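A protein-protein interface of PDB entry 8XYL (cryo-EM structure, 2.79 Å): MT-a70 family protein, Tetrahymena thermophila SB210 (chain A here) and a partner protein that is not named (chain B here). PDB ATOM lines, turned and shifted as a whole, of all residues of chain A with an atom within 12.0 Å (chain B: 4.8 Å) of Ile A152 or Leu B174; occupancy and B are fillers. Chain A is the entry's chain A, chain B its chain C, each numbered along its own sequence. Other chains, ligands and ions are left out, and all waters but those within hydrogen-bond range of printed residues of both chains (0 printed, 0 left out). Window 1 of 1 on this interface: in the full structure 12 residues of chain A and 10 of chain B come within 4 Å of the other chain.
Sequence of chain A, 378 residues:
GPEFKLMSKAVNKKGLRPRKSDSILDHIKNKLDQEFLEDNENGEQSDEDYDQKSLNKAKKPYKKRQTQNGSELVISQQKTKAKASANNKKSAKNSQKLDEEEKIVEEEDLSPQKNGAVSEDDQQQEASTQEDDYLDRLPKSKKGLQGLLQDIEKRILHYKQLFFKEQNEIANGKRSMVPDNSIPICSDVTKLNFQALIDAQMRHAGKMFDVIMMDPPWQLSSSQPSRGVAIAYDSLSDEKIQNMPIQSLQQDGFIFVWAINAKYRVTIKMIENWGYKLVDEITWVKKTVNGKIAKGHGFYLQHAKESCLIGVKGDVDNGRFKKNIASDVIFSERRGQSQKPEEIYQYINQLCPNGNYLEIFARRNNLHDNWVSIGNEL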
ATOM      1  N   LYS A 143     -36.198   9.949  13.608  1.00  0.00           N
ATOM      2  CA  LYS A 143     -34.784  10.267  13.775  1.00  0.00           C
ATOM      3  C   LYS A 143     -34.368  10.211  15.239  1.00  0.00           C
ATOM      4  O   LYS A 143     -33.175  10.082  15.538  1.00  0.00           O
ATOM      5  CB  LYS A 143     -34.479  11.643  13.184  1.00  0.00           C
ATOM      6  CG  LYS A 143     -34.590  11.700  11.669  1.00  0.00           C
ATOM      7  CD  LYS A 143     -34.260  13.086  11.138  1.00  0.00           C
ATOM      8  CE  LYS A 143     -34.325  13.124   9.620  1.00  0.00           C
ATOM      9  NZ  LYS A 143     -34.022  14.478   9.080  1.00  0.00           N
ATOM     10  N   GLY A 144     -35.330  10.314  16.160  1.00  0.00           N
ATOM     11  CA  GLY A 144     -35.017  10.151  17.569  1.00  0.00           C
ATOM     12  C   GLY A 144     -34.554   8.749  17.911  1.00  0.00           C
ATOM     13  O   GLY A 144     -33.680   8.569  18.763  1.00  0.00           O
ATOM     14  N   LEU A 145     -35.120   7.740  17.247  1.00  0.00           N
ATOM     15  CA  LEU A 145     -34.648   6.374  17.441  1.00  0.00           C
ATOM     16  C   LEU A 145     -33.232   6.202  16.905  1.00  0.00           C
ATOM     17  O   LEU A 145     -32.421   5.479  17.495  1.00  0.00           O
ATOM     18  CB  LEU A 145     -35.608   5.387  16.776  1.00  0.00           C
ATOM     19  CG  LEU A 145     -35.437   3.911  17.143  1.00  0.00           C
ATOM     20  CD1 LEU A 145     -35.290   3.743  18.648  1.00  0.00           C
ATOM     21  CD2 LEU A 145     -36.605   3.089  16.621  1.00  0.00           C
ATOM     22  N   GLN A 146     -32.910   6.870  15.793  1.00  0.00           N
ATOM     23  CA  GLN A 146     -31.542   6.839  15.280  1.00  0.00           C
ATOM     24  C   GLN A 146     -30.580   7.541  16.232  1.00  0.00           C
ATOM     25  O   GLN A 146     -29.436   7.104  16.405  1.00  0.00           O
ATOM     26  CB  GLN A 146     -31.486   7.474  13.892  1.00  0.00           C
ATOM     27  CG  GLN A 146     -32.373   6.794  12.864  1.00  0.00           C
ATOM     28  CD  GLN A 146     -32.792   7.731  11.750  1.00  0.00           C
ATOM     29  OE1 GLN A 146     -33.945   7.726  11.320  1.00  0.00           O
ATOM     30  NE2 GLN A 146     -31.853   8.540  11.274  1.00  0.00           N
ATOM     31  N   GLY A 147     -31.023   8.636  16.853  1.00  0.00           N
ATOM     32  CA  GLY A 147     -30.208   9.275  17.874  1.00  0.00           C
ATOM     33  C   GLY A 147     -30.001   8.397  19.092  1.00  0.00           C
ATOM     34  O   GLY A 147     -28.920   8.398  19.688  1.00  0.00           O
ATOM     35  N   LEU A 148     -31.029   7.638  19.476  1.00  0.00           N
ATOM     36  CA  LEU A 148     -30.878   6.665  20.554  1.00  0.00           C
ATOM     37  C   LEU A 148     -29.891   5.570  20.163  1.00  0.00           C
ATOM     38  O   LEU A 148     -29.116   5.095  21.001  1.00  0.00           O
ATOM     39  CB  LEU A 148     -32.247   6.079  20.915  1.00  0.00           C
ATOM     40  CG  LEU A 148     -32.434   5.137  22.113  1.00  0.00           C
ATOM     41  CD1 LEU A 148     -32.274   3.667  21.734  1.00  0.00           C
ATOM     42  CD2 LEU A 148     -31.504   5.510  23.261  1.00  0.00           C
ATOM     43  N   LEU A 149     -29.914   5.157  18.893  1.00  0.00           N
ATOM     44  CA  LEU A 149     -28.934   4.195  18.397  1.00  0.00           C
ATOM     45  C   LEU A 149     -27.521   4.759  18.475  1.00  0.00           C
ATOM     46  O   LEU A 149     -26.581   4.051  18.856  1.00  0.00           O
ATOM     47  CB  LEU A 149     -29.274   3.802  16.958  1.00  0.00           C
ATOM     48  CG  LEU A 149     -28.314   2.885  16.197  1.00  0.00           C
ATOM     49  CD1 LEU A 149     -28.006   1.630  16.994  1.00  0.00           C
ATOM     50  CD2 LEU A 149     -28.897   2.524  14.840  1.00  0.00           C
ATOM     51  N   GLN A 150     -27.354   6.034  18.121  1.00  0.00           N
ATOM     52  CA  GLN A 150     -26.047   6.672  18.239  1.00  0.00           C
ATOM     53  C   GLN A 150     -25.587   6.724  19.693  1.00  0.00           C
ATOM     54  O   GLN A 150     -24.422   6.434  19.995  1.00  0.00           O
ATOM     55  CB  GLN A 150     -26.090   8.080  17.642  1.00  0.00           C
ATOM     56  CG  GLN A 150     -26.322   8.148  16.133  1.00  0.00           C
ATOM     57  CD  GLN A 150     -25.792   6.939  15.382  1.00  0.00           C
ATOM     58  OE1 GLN A 150     -26.523   5.981  15.124  1.00  0.00           O
ATOM     59  NE2 GLN A 150     -24.513   6.978  15.026  1.00  0.00           N
ATOM     60  N   ASP A 151     -26.498   7.080  20.605  1.00  0.00           N
ATOM     61  CA  ASP A 151     -26.155   7.147  22.023  1.00  0.00           C
ATOM     62  C   ASP A 151     -25.758   5.780  22.567  1.00  0.00           C
ATOM     63  O   ASP A 151     -24.777   5.659  23.313  1.00  0.00           O
ATOM     64  CB  ASP A 151     -27.330   7.716  22.819  1.00  0.00           C
ATOM     65  CG  ASP A 151     -26.992   7.945  24.280  1.00  0.00           C
ATOM     66  OD1 ASP A 151     -25.795   8.097  24.604  1.00  0.00           O
ATOM     67  OD2 ASP A 151     -27.926   7.972  25.108  1.00  0.00           O
ATOM     68  N   ILE A 152     -26.503   4.734  22.198  1.00  0.00           N
ATOM     69  CA  ILE A 152     -26.147   3.394  22.644  1.00  0.00           C
ATOM     70  C   ILE A 152     -24.850   2.929  21.990  1.00  0.00           C
ATOM     71  O   ILE A 152     -24.120   2.136  22.588  1.00  0.00           O
ATOM     72  CB  ILE A 152     -27.314   2.408  22.409  1.00  0.00           C
ATOM     73  CG1 ILE A 152     -27.307   1.314  23.477  1.00  0.00           C
ATOM     74  CG2 ILE A 152     -27.267   1.773  21.032  1.00  0.00           C
ATOM     75  CD1 ILE A 152     -27.532   1.829  24.877  1.00  0.00           C
ATOM     76  N   GLU A 153     -24.517   3.439  20.801  1.00  0.00           N
ATOM     77  CA  GLU A 153     -23.228   3.119  20.193  1.00  0.00           C
ATOM     78  C   GLU A 153     -22.079   3.729  20.986  1.00  0.00           C
ATOM     79  O   GLU A 153     -21.063   3.065  21.233  1.00  0.00           O
ATOM     80  CB  GLU A 153     -23.199   3.599  18.742  1.00  0.00           C
ATOM     81  CG  GLU A 153     -21.970   3.156  17.971  1.00  0.00           C
ATOM     82  CD  GLU A 153     -22.093   3.413  16.482  1.00  0.00           C
ATOM     83  OE1 GLU A 153     -23.114   3.997  16.060  1.00  0.00           O
ATOM     84  OE2 GLU A 153     -21.168   3.033  15.734  1.00  0.00           O
ATOM     85  N   LYS A 154     -22.216   4.998  21.391  1.00  0.00           N
ATOM     86  CA  LYS A 154     -21.174   5.610  22.218  1.00  0.00           C
ATOM     87  C   LYS A 154     -21.066   4.919  23.572  1.00  0.00           C
ATOM     88  O   LYS A 154     -19.961   4.748  24.102  1.00  0.00           O
ATOM     89  CB  LYS A 154     -21.405   7.110  22.419  1.00  0.00           C
ATOM     90  CG  LYS A 154     -22.012   7.862  21.261  1.00  0.00           C
ATOM     91  CD  LYS A 154     -21.098   7.874  20.045  1.00  0.00           C
ATOM     92  CE  LYS A 154     -21.735   8.636  18.893  1.00  0.00           C
ATOM     93  NZ  LYS A 154     -21.181   8.223  17.574  1.00  0.00           N
ATOM     94  N   ARG A 155     -22.202   4.520  24.152  1.00  0.00           N
ATOM     95  CA  ARG A 155     -22.166   3.799  25.421  1.00  0.00           C
ATOM     96  C   ARG A 155     -21.489   2.441  25.273  1.00  0.00           C
ATOM     97  O   ARG A 155     -20.705   2.030  26.140  1.00  0.00           O
ATOM     98  CB  ARG A 155     -23.583   3.647  25.972  1.00  0.00           C
ATOM     99  CG  ARG A 155     -24.196   4.955  26.450  1.00  0.00           C
ATOM    100  CD  ARG A 155     -23.582   5.409  27.765  1.00  0.00           C
ATOM    101  NE  ARG A 155     -22.492   6.357  27.575  1.00  0.00           N
ATOM    102  CZ  ARG A 155     -21.704   6.797  28.547  1.00  0.00           C
ATOM    103  NH1 ARG A 155     -21.862   6.397  29.799  1.00  0.00           N
ATOM    104  NH2 ARG A 155     -20.735   7.659  28.257  1.00  0.00           N
ATOM    105  N   ILE A 156     -21.768   1.738  24.170  1.00  0.00           N
ATOM    106  CA  ILE A 156     -21.126   0.455  23.899  1.00  0.00           C
ATOM    107  C   ILE A 156     -19.624   0.634  23.735  1.00  0.00           C
ATOM    108  O   ILE A 156     -18.836  -0.156  24.261  1.00  0.00           O
ATOM    109  CB  ILE A 156     -21.769  -0.213  22.666  1.00  0.00           C
ATOM    110  CG1 ILE A 156     -22.908  -1.134  23.096  1.00  0.00           C
ATOM    111  CG2 ILE A 156     -20.756  -1.001  21.846  1.00  0.00           C
ATOM    112  CD1 ILE A 156     -23.679  -1.724  21.947  1.00  0.00           C
ATOM    113  N   LEU A 157     -19.202   1.685  23.024  1.00  0.00           N
ATOM    114  CA  LEU A 157     -17.771   1.926  22.842  1.00  0.00           C
ATOM    115  C   LEU A 157     -17.085   2.278  24.158  1.00  0.00           C
ATOM    116  O   LEU A 157     -15.977   1.797  24.435  1.00  0.00           O
ATOM    117  CB  LEU A 157     -17.554   3.028  21.808  1.00  0.00           C
ATOM    118  CG  LEU A 157     -17.501   2.548  20.359  1.00  0.00           C
ATOM    119  CD1 LEU A 157     -17.398   3.723  19.402  1.00  0.00           C
ATOM    120  CD2 LEU A 157     -16.333   1.594  20.170  1.00  0.00           C
ATOM    121  N   HIS A 158     -17.731   3.103  24.988  1.00  0.00           N
ATOM    122  CA  HIS A 158     -17.156   3.467  26.281  1.00  0.00           C
ATOM    123  C   HIS A 158     -17.007   2.248  27.182  1.00  0.00           C
ATOM    124  O   HIS A 158     -15.951   2.034  27.795  1.00  0.00           O
ATOM    125  CB  HIS A 158     -18.028   4.528  26.952  1.00  0.00           C
ATOM    126  CG  HIS A 158     -17.553   4.931  28.314  1.00  0.00           C
ATOM    127  ND1 HIS A 158     -18.418   5.205  29.351  1.00  0.00           N
ATOM    128  CD2 HIS A 158     -16.306   5.116  28.806  1.00  0.00           C
ATOM    129  CE1 HIS A 158     -17.724   5.536  30.426  1.00  0.00           C
ATOM    130  NE2 HIS A 158     -16.440   5.491  30.121  1.00  0.00           N
ATOM    131  N   TYR A 159     -18.047   1.416  27.255  1.00  0.00           N
ATOM    132  CA  TYR A 159     -17.974   0.253  28.128  1.00  0.00           C
ATOM    133  C   TYR A 159     -17.076  -0.833  27.548  1.00  0.00           C
ATOM    134  O   TYR A 159     -16.478  -1.602  28.305  1.00  0.00           O
ATOM    135  CB  TYR A 159     -19.378  -0.275  28.416  1.00  0.00           C
ATOM    136  CG  TYR A 159     -20.059   0.480  29.532  1.00  0.00           C
ATOM    137  CD1 TYR A 159     -19.594   0.396  30.836  1.00  0.00           C
ATOM    138  CD2 TYR A 159     -21.153   1.298  29.278  1.00  0.00           C
ATOM    139  CE1 TYR A 159     -20.205   1.092  31.860  1.00  0.00           C
ATOM    140  CE2 TYR A 159     -21.771   2.000  30.297  1.00  0.00           C
ATOM    141  CZ  TYR A 159     -21.292   1.892  31.585  1.00  0.00           C
ATOM    142  OH  TYR A 159     -21.904   2.587  32.604  1.00  0.00           O
ATOM    143  N   LYS A 160     -16.942  -0.894  26.221  1.00  0.00           N
ATOM    144  CA  LYS A 160     -15.959  -1.778  25.605  1.00  0.00           C
ATOM    145  C   LYS A 160     -14.546  -1.365  25.982  1.00  0.00           C
ATOM    146  O   LYS A 160     -13.702  -2.216  26.286  1.00  0.00           O
ATOM    147  CB  LYS A 160     -16.128  -1.769  24.087  1.00  0.00           C
ATOM    148  CG  LYS A 160     -15.616  -3.014  23.392  1.00  0.00           C
ATOM    149  CD  LYS A 160     -16.046  -3.065  21.933  1.00  0.00           C
ATOM    150  CE  LYS A 160     -17.541  -2.874  21.772  1.00  0.00           C
ATOM    151  NZ  LYS A 160     -18.323  -3.829  22.603  1.00  0.00           N
ATOM    152  N   GLN A 161     -14.272  -0.058  25.967  1.00  0.00           N
ATOM    153  CA  GLN A 161     -12.963   0.429  26.391  1.00  0.00           C
ATOM    154  C   GLN A 161     -12.708   0.123  27.861  1.00  0.00           C
ATOM    155  O   GLN A 161     -11.594  -0.259  28.237  1.00  0.00           O
ATOM    156  CB  GLN A 161     -12.848   1.930  26.126  1.00  0.00           C
ATOM    157  CG  GLN A 161     -11.434   2.392  25.824  1.00  0.00           C
ATOM    158  CD  GLN A 161     -10.669   1.405  24.966  1.00  0.00           C
ATOM    159  OE1 GLN A 161      -9.704   0.791  25.419  1.00  0.00           O
ATOM    160  NE2 GLN A 161     -11.090   1.255  23.714  1.00  0.00           N
ATOM    161  N   LEU A 162     -13.728   0.285  28.708  1.00  0.00           N
ATOM    162  CA  LEU A 162     -13.562  -0.038  30.125  1.00  0.00           C
ATOM    163  C   LEU A 162     -13.327  -1.531  30.342  1.00  0.00           C
ATOM    164  O   LEU A 162     -12.498  -1.920  31.176  1.00  0.00           O
ATOM    165  CB  LEU A 162     -14.777   0.432  30.920  1.00  0.00           C
ATOM    166  CG  LEU A 162     -15.009   1.937  31.026  1.00  0.00           C
ATOM    167  CD1 LEU A 162     -16.495   2.228  31.039  1.00  0.00           C
ATOM    168  CD2 LEU A 162     -14.337   2.489  32.271  1.00  0.00           C
ATOM    169  N   PHE A 163     -14.049  -2.382  29.607  1.00  0.00           N
ATOM    170  CA  PHE A 163     -13.851  -3.824  29.708  1.00  0.00           C
ATOM    171  C   PHE A 163     -12.452  -4.220  29.255  1.00  0.00           C
ATOM    172  O   PHE A 163     -11.796  -5.054  29.888  1.00  0.00           O
ATOM    173  CB  PHE A 163     -14.918  -4.552  28.884  1.00  0.00           C
ATOM    174  CG  PHE A 163     -14.713  -6.040  28.788  1.00  0.00           C
ATOM    175  CD1 PHE A 163     -15.071  -6.873  29.834  1.00  0.00           C
ATOM    176  CD2 PHE A 163     -14.183  -6.606  27.640  1.00  0.00           C
ATOM    177  CE1 PHE A 163     -14.889  -8.238  29.743  1.00  0.00           C
ATOM    178  CE2 PHE A 163     -13.999  -7.970  27.546  1.00  0.00           C
ATOM    179  CZ  PHE A 163     -14.354  -8.786  28.598  1.00  0.00           C
ATOM    180  N   LEU B 157     -31.921   2.326  29.358  1.00  0.00           N
ATOM    181  CA  LEU B 157     -30.467   2.315  29.220  1.00  0.00           C
ATOM    182  C   LEU B 157     -29.795   3.091  30.346  1.00  0.00           C
ATOM    183  O   LEU B 157     -28.752   2.676  30.864  1.00  0.00           O
ATOM    184  CB  LEU B 157     -30.057   2.873  27.853  1.00  0.00           C
ATOM    185  CG  LEU B 157     -30.497   4.264  27.383  1.00  0.00           C
ATOM    186  CD1 LEU B 157     -29.473   4.808  26.404  1.00  0.00           C
ATOM    187  CD2 LEU B 157     -31.874   4.241  26.732  1.00  0.00           C
ATOM    188  N   ILE B 160     -29.635   0.851  33.443  1.00  0.00           N
ATOM    189  CA  ILE B 160     -28.681  -0.256  33.444  1.00  0.00           C
ATOM    190  C   ILE B 160     -27.249   0.264  33.420  1.00  0.00           C
ATOM    191  O   ILE B 160     -26.317  -0.426  33.848  1.00  0.00           O
ATOM    192  CB  ILE B 160     -28.961  -1.220  32.273  1.00  0.00           C
ATOM    193  CG1 ILE B 160     -28.645  -0.563  30.925  1.00  0.00           C
ATOM    194  CG2 ILE B 160     -30.404  -1.716  32.334  1.00  0.00           C
ATOM    195  CD1 ILE B 160     -29.253  -1.264  29.722  1.00  0.00           C
ATOM    196  N   GLU B 161     -27.045   1.488  32.922  1.00  0.00           N
ATOM    197  CA  GLU B 161     -25.696   2.043  32.882  1.00  0.00           C
ATOM    198  C   GLU B 161     -25.245   2.505  34.261  1.00  0.00           C
ATOM    199  O   GLU B 161     -24.070   2.362  34.619  1.00  0.00           O
ATOM    200  CB  GLU B 161     -25.633   3.190  31.876  1.00  0.00           C
ATOM    201  CG  GLU B 161     -25.559   2.723  30.434  1.00  0.00           C
ATOM    202  CD  GLU B 161     -26.194   3.703  29.473  1.00  0.00           C
ATOM    203  OE1 GLU B 161     -26.605   4.794  29.917  1.00  0.00           O
ATOM    204  OE2 GLU B 161     -26.304   3.372  28.275  1.00  0.00           O
ATOM    205  N   ILE B 170     -23.604  -5.246  31.569  1.00  0.00           N
ATOM    206  CA  ILE B 170     -23.947  -3.963  30.958  1.00  0.00           C
ATOM    207  C   ILE B 170     -23.738  -4.027  29.452  1.00  0.00           C
ATOM    208  O   ILE B 170     -24.579  -3.565  28.670  1.00  0.00           O
ATOM    209  CB  ILE B 170     -23.116  -2.833  31.601  1.00  0.00           C
ATOM    210  CG1 ILE B 170     -23.761  -2.360  32.901  1.00  0.00           C
ATOM    211  CG2 ILE B 170     -22.953  -1.656  30.651  1.00  0.00           C
ATOM    212  CD1 ILE B 170     -22.831  -1.555  33.783  1.00  0.00           C
ATOM    213  N   LEU B 171     -22.628  -4.635  29.024  1.00  0.00           N
ATOM    214  CA  LEU B 171     -22.288  -4.689  27.607  1.00  0.00           C
ATOM    215  C   LEU B 171     -23.280  -5.552  26.831  1.00  0.00           C
ATOM    216  O   LEU B 171     -23.708  -5.178  25.732  1.00  0.00           O
ATOM    217  CB  LEU B 171     -20.857  -5.210  27.459  1.00  0.00           C
ATOM    218  CG  LEU B 171     -19.943  -4.780  26.307  1.00  0.00           C
ATOM    219  CD1 LEU B 171     -20.434  -5.226  24.951  1.00  0.00           C
ATOM    220  CD2 LEU B 171     -19.751  -3.273  26.330  1.00  0.00           C
ATOM    221  N   THR B 172     -23.679  -6.697  27.393  1.00  0.00           N
ATOM    222  CA  THR B 172     -24.623  -7.547  26.671  1.00  0.00           C
ATOM    223  C   THR B 172     -26.042  -6.985  26.716  1.00  0.00           C
ATOM    224  O   THR B 172     -26.797  -7.160  25.753  1.00  0.00           O
ATOM    225  CB  THR B 172     -24.593  -8.989  27.190  1.00  0.00           C
ATOM    226  OG1 THR B 172     -25.559  -9.769  26.475  1.00  0.00           O
ATOM    227  CG2 THR B 172     -24.918  -9.063  28.657  1.00  0.00           C
ATOM    228  N   HIS B 173     -26.419  -6.287  27.796  1.00  0.00           N
ATOM    229  CA  HIS B 173     -27.698  -5.583  27.804  1.00  0.00           C
ATOM    230  C   HIS B 173     -27.720  -4.487  26.749  1.00  0.00           C
ATOM    231  O   HIS B 173     -28.726  -4.301  26.054  1.00  0.00           O
ATOM    232  CB  HIS B 173     -27.969  -4.993  29.187  1.00  0.00           C
ATOM    233  CG  HIS B 173     -28.418  -5.998  30.200  1.00  0.00           C
ATOM    234  ND1 HIS B 173     -28.250  -5.814  31.556  1.00  0.00           N
ATOM    235  CD2 HIS B 173     -29.031  -7.198  30.057  1.00  0.00           C
ATOM    236  CE1 HIS B 173     -28.737  -6.857  32.204  1.00  0.00           C
ATOM    237  NE2 HIS B 173     -29.216  -7.710  31.318  1.00  0.00           N
ATOM    238  N   LEU B 174     -26.610  -3.757  26.615  1.00  0.00           N
ATOM    239  CA  LEU B 174     -26.505  -2.714  25.602  1.00  0.00           C
ATOM    240  C   LEU B 174     -26.593  -3.301  24.198  1.00  0.00           C
ATOM    241  O   LEU B 174     -27.252  -2.738  23.317  1.00  0.00           O
ATOM    242  CB  LEU B 174     -25.195  -1.951  25.792  1.00  0.00           C
ATOM    243  CG  LEU B 174     -25.210  -0.603  26.519  1.00  0.00           C
ATOM    244  CD1 LEU B 174     -26.017  -0.670  27.804  1.00  0.00           C
ATOM    245  CD2 LEU B 174     -23.789  -0.148  26.812  1.00  0.00           C
ATOM    246  N   TYR B 175     -25.934  -4.444  23.976  1.00  0.00           N
ATOM    247  CA  TYR B 175     -25.999  -5.096  22.669  1.00  0.00           C
ATOM    248  C   TYR B 175     -27.405  -5.595  22.357  1.00  0.00           C
ATOM    249  O   TYR B 175     -27.875  -5.469  21.221  1.00  0.00           O
ATOM    250  CB  TYR B 175     -24.995  -6.245  22.599  1.00  0.00           C
ATOM    251  CG  TYR B 175     -23.789  -5.940  21.742  1.00  0.00           C
ATOM    252  CD1 TYR B 175     -23.781  -6.240  20.387  1.00  0.00           C
ATOM    253  CD2 TYR B 175     -22.666  -5.339  22.285  1.00  0.00           C
ATOM    254  CE1 TYR B 175     -22.678  -5.955  19.599  1.00  0.00           C
ATOM    255  CE2 TYR B 175     -21.561  -5.051  21.510  1.00  0.00           C
ATOM    256  CZ  TYR B 175     -21.571  -5.359  20.168  1.00  0.00           C
ATOM    257  OH  TYR B 175     -20.471  -5.072  19.394  1.00  0.00           O
ATOM    258  N   ASN B 176     -28.090  -6.169  23.351  1.00  0.00           N
ATOM    259  CA  ASN B 176     -29.458  -6.636  23.138  1.00  0.00           C
ATOM    260  C   ASN B 176     -30.392  -5.473  22.829  1.00  0.00           C
ATOM    261  O   ASN B 176     -31.242  -5.564  21.932  1.00  0.00           O
ATOM    262  CB  ASN B 176     -29.944  -7.408  24.365  1.00  0.00           C
ATOM    263  CG  ASN B 176     -29.471  -8.847  24.372  1.00  0.00           C
ATOM    264  OD1 ASN B 176     -28.971  -9.342  25.382  1.00  0.00           O
ATOM    265  ND2 ASN B 176     -29.627  -9.527  23.242  1.00  0.00           N
ATOM    266  N   LEU B 177     -30.239  -4.363  23.560  1.00  0.00           N
ATOM    267  CA  LEU B 177     -31.054  -3.180  23.307  1.00  0.00           C
ATOM    268  C   LEU B 177     -30.793  -2.625  21.912  1.00  0.00           C
ATOM    269  O   LEU B 177     -31.739  -2.272  21.196  1.00  0.00           O
ATOM    270  CB  LEU B 177     -30.774  -2.123  24.381  1.00  0.00           C
ATOM    271  CG  LEU B 177     -31.702  -0.920  24.613  1.00  0.00           C
ATOM    272  CD1 LEU B 177     -31.494  -0.398  26.024  1.00  0.00           C
ATOM    273  CD2 LEU B 177     -31.490   0.216  23.617  1.00  0.00           C
ATOM    274  N   LYS B 178     -29.519  -2.553  21.507  1.00  0.00           N
ATOM    275  CA  LYS B 178     -29.181  -2.049  20.178  1.00  0.00           C
ATOM    276  C   LYS B 178     -29.752  -2.944  19.085  1.00  0.00           C
ATOM    277  O   LYS B 178     -30.295  -2.447  18.091  1.00  0.00           O
ATOM    278  CB  LYS B 178     -27.661  -1.918  20.037  1.00  0.00           C
ATOM    279  CG  LYS B 178     -27.129  -2.201  18.634  1.00  0.00           C
ATOM    280  CD  LYS B 178     -25.622  -2.400  18.624  1.00  0.00           C
ATOM    281  CE  LYS B 178     -24.890  -1.071  18.556  1.00  0.00           C
ATOM    282  NZ  LYS B 178     -25.222  -0.308  17.322  1.00  0.00           N
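Among the printed residues, pairs that only touch across the chains: Arg A155 with Glu B161 (3.2 Å), Leu A149 with Lys B178 (3.4 Å), Lys A160 with Leu B171 (3.5 Å), Ile A156 with Leu B174 (3.6 Å), Lys A160 with Tyr B175 (3.6 Å), Ile A156 with Lys B178 (3.7 Å), Tyr A159 with Leu B171 (3.7 Å), Leu A148 with Leu B157 (3.7 Å), Tyr A159 with Ile B170 (3.7 Å), Ile A152 with Leu B174 (3.7 Å), Asp A151 with Leu B157 (3.8 Å), Ile A156 with Tyr B175 (3.8 Å), Arg A155 with Leu B174 (3.8 Å), Ile A152 with Lys B178 (3.8 Å), Ile A156 with Leu B171 (3.9 Å), Ile A152 with Leu B157 (3.9 Å), Tyr A159 with Leu B174 (3.9 Å) and Ile A152 with Glu B161 (3.9 Å).
OH of Tyr A159 is in hydrogen-bond range of O of Glu B161.
Leu B174 touches just these residues of chain A: Ile A152 (3.7 Å), Arg A155 (3.8 Å), Ile A156 (3.6 Å) and Tyr A159 (3.9 Å). Of chain A, only Leu A148 (3.7 Å), Asp A151 (3.8 Å) and Ile A152 (3.9 Å) come within 4 Å of Leu B157. Of chain A, only Ile A152 (3.9 Å), Arg A155 (3.2 Å) and Tyr A159 (3.0 Å) come within 4 Å of Glu B161. Of chain A, only Tyr A159 (3.7 Å) comes within 4 Å of Ile B170. Of chain A, only Ile A156, Tyr A159 and Lys A160 come within 4 Å of Leu B171. Thr B172 touches none of the printed residues of chain A. No residue of chain A comes within 4 Å of His B173. No residue of chain A comes within 4 Å of Asn B176. Lys B178 touches just these residues of chain A: Leu A149 (3.4 Å), Ile A152 (3.8 Å) and Ile A156 (3.7 Å). Printed residues of chain B within 4 Å of Lys A160: Leu B171 (3.5 Å) and Tyr B175 (3.6 Å). Of the printed residues of chain B, Leu A148 touches Leu B157. Of the printed residues of chain B, Tyr A159 touches Glu B161, Ile B170, Leu B171 and Leu B174. Of the printed residues of chain B, Arg A155 touches Glu B161 and Leu B174. Of the printed residues of chain B, Leu A149 touches Lys B178 (3.4 Å). The nearest residue of chain B that does not touch Ile A152 is Leu B177 (4.3 Å). The nearest printed residue of chain B that does not touch Arg A155 is Leu B157 (5.3 Å).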
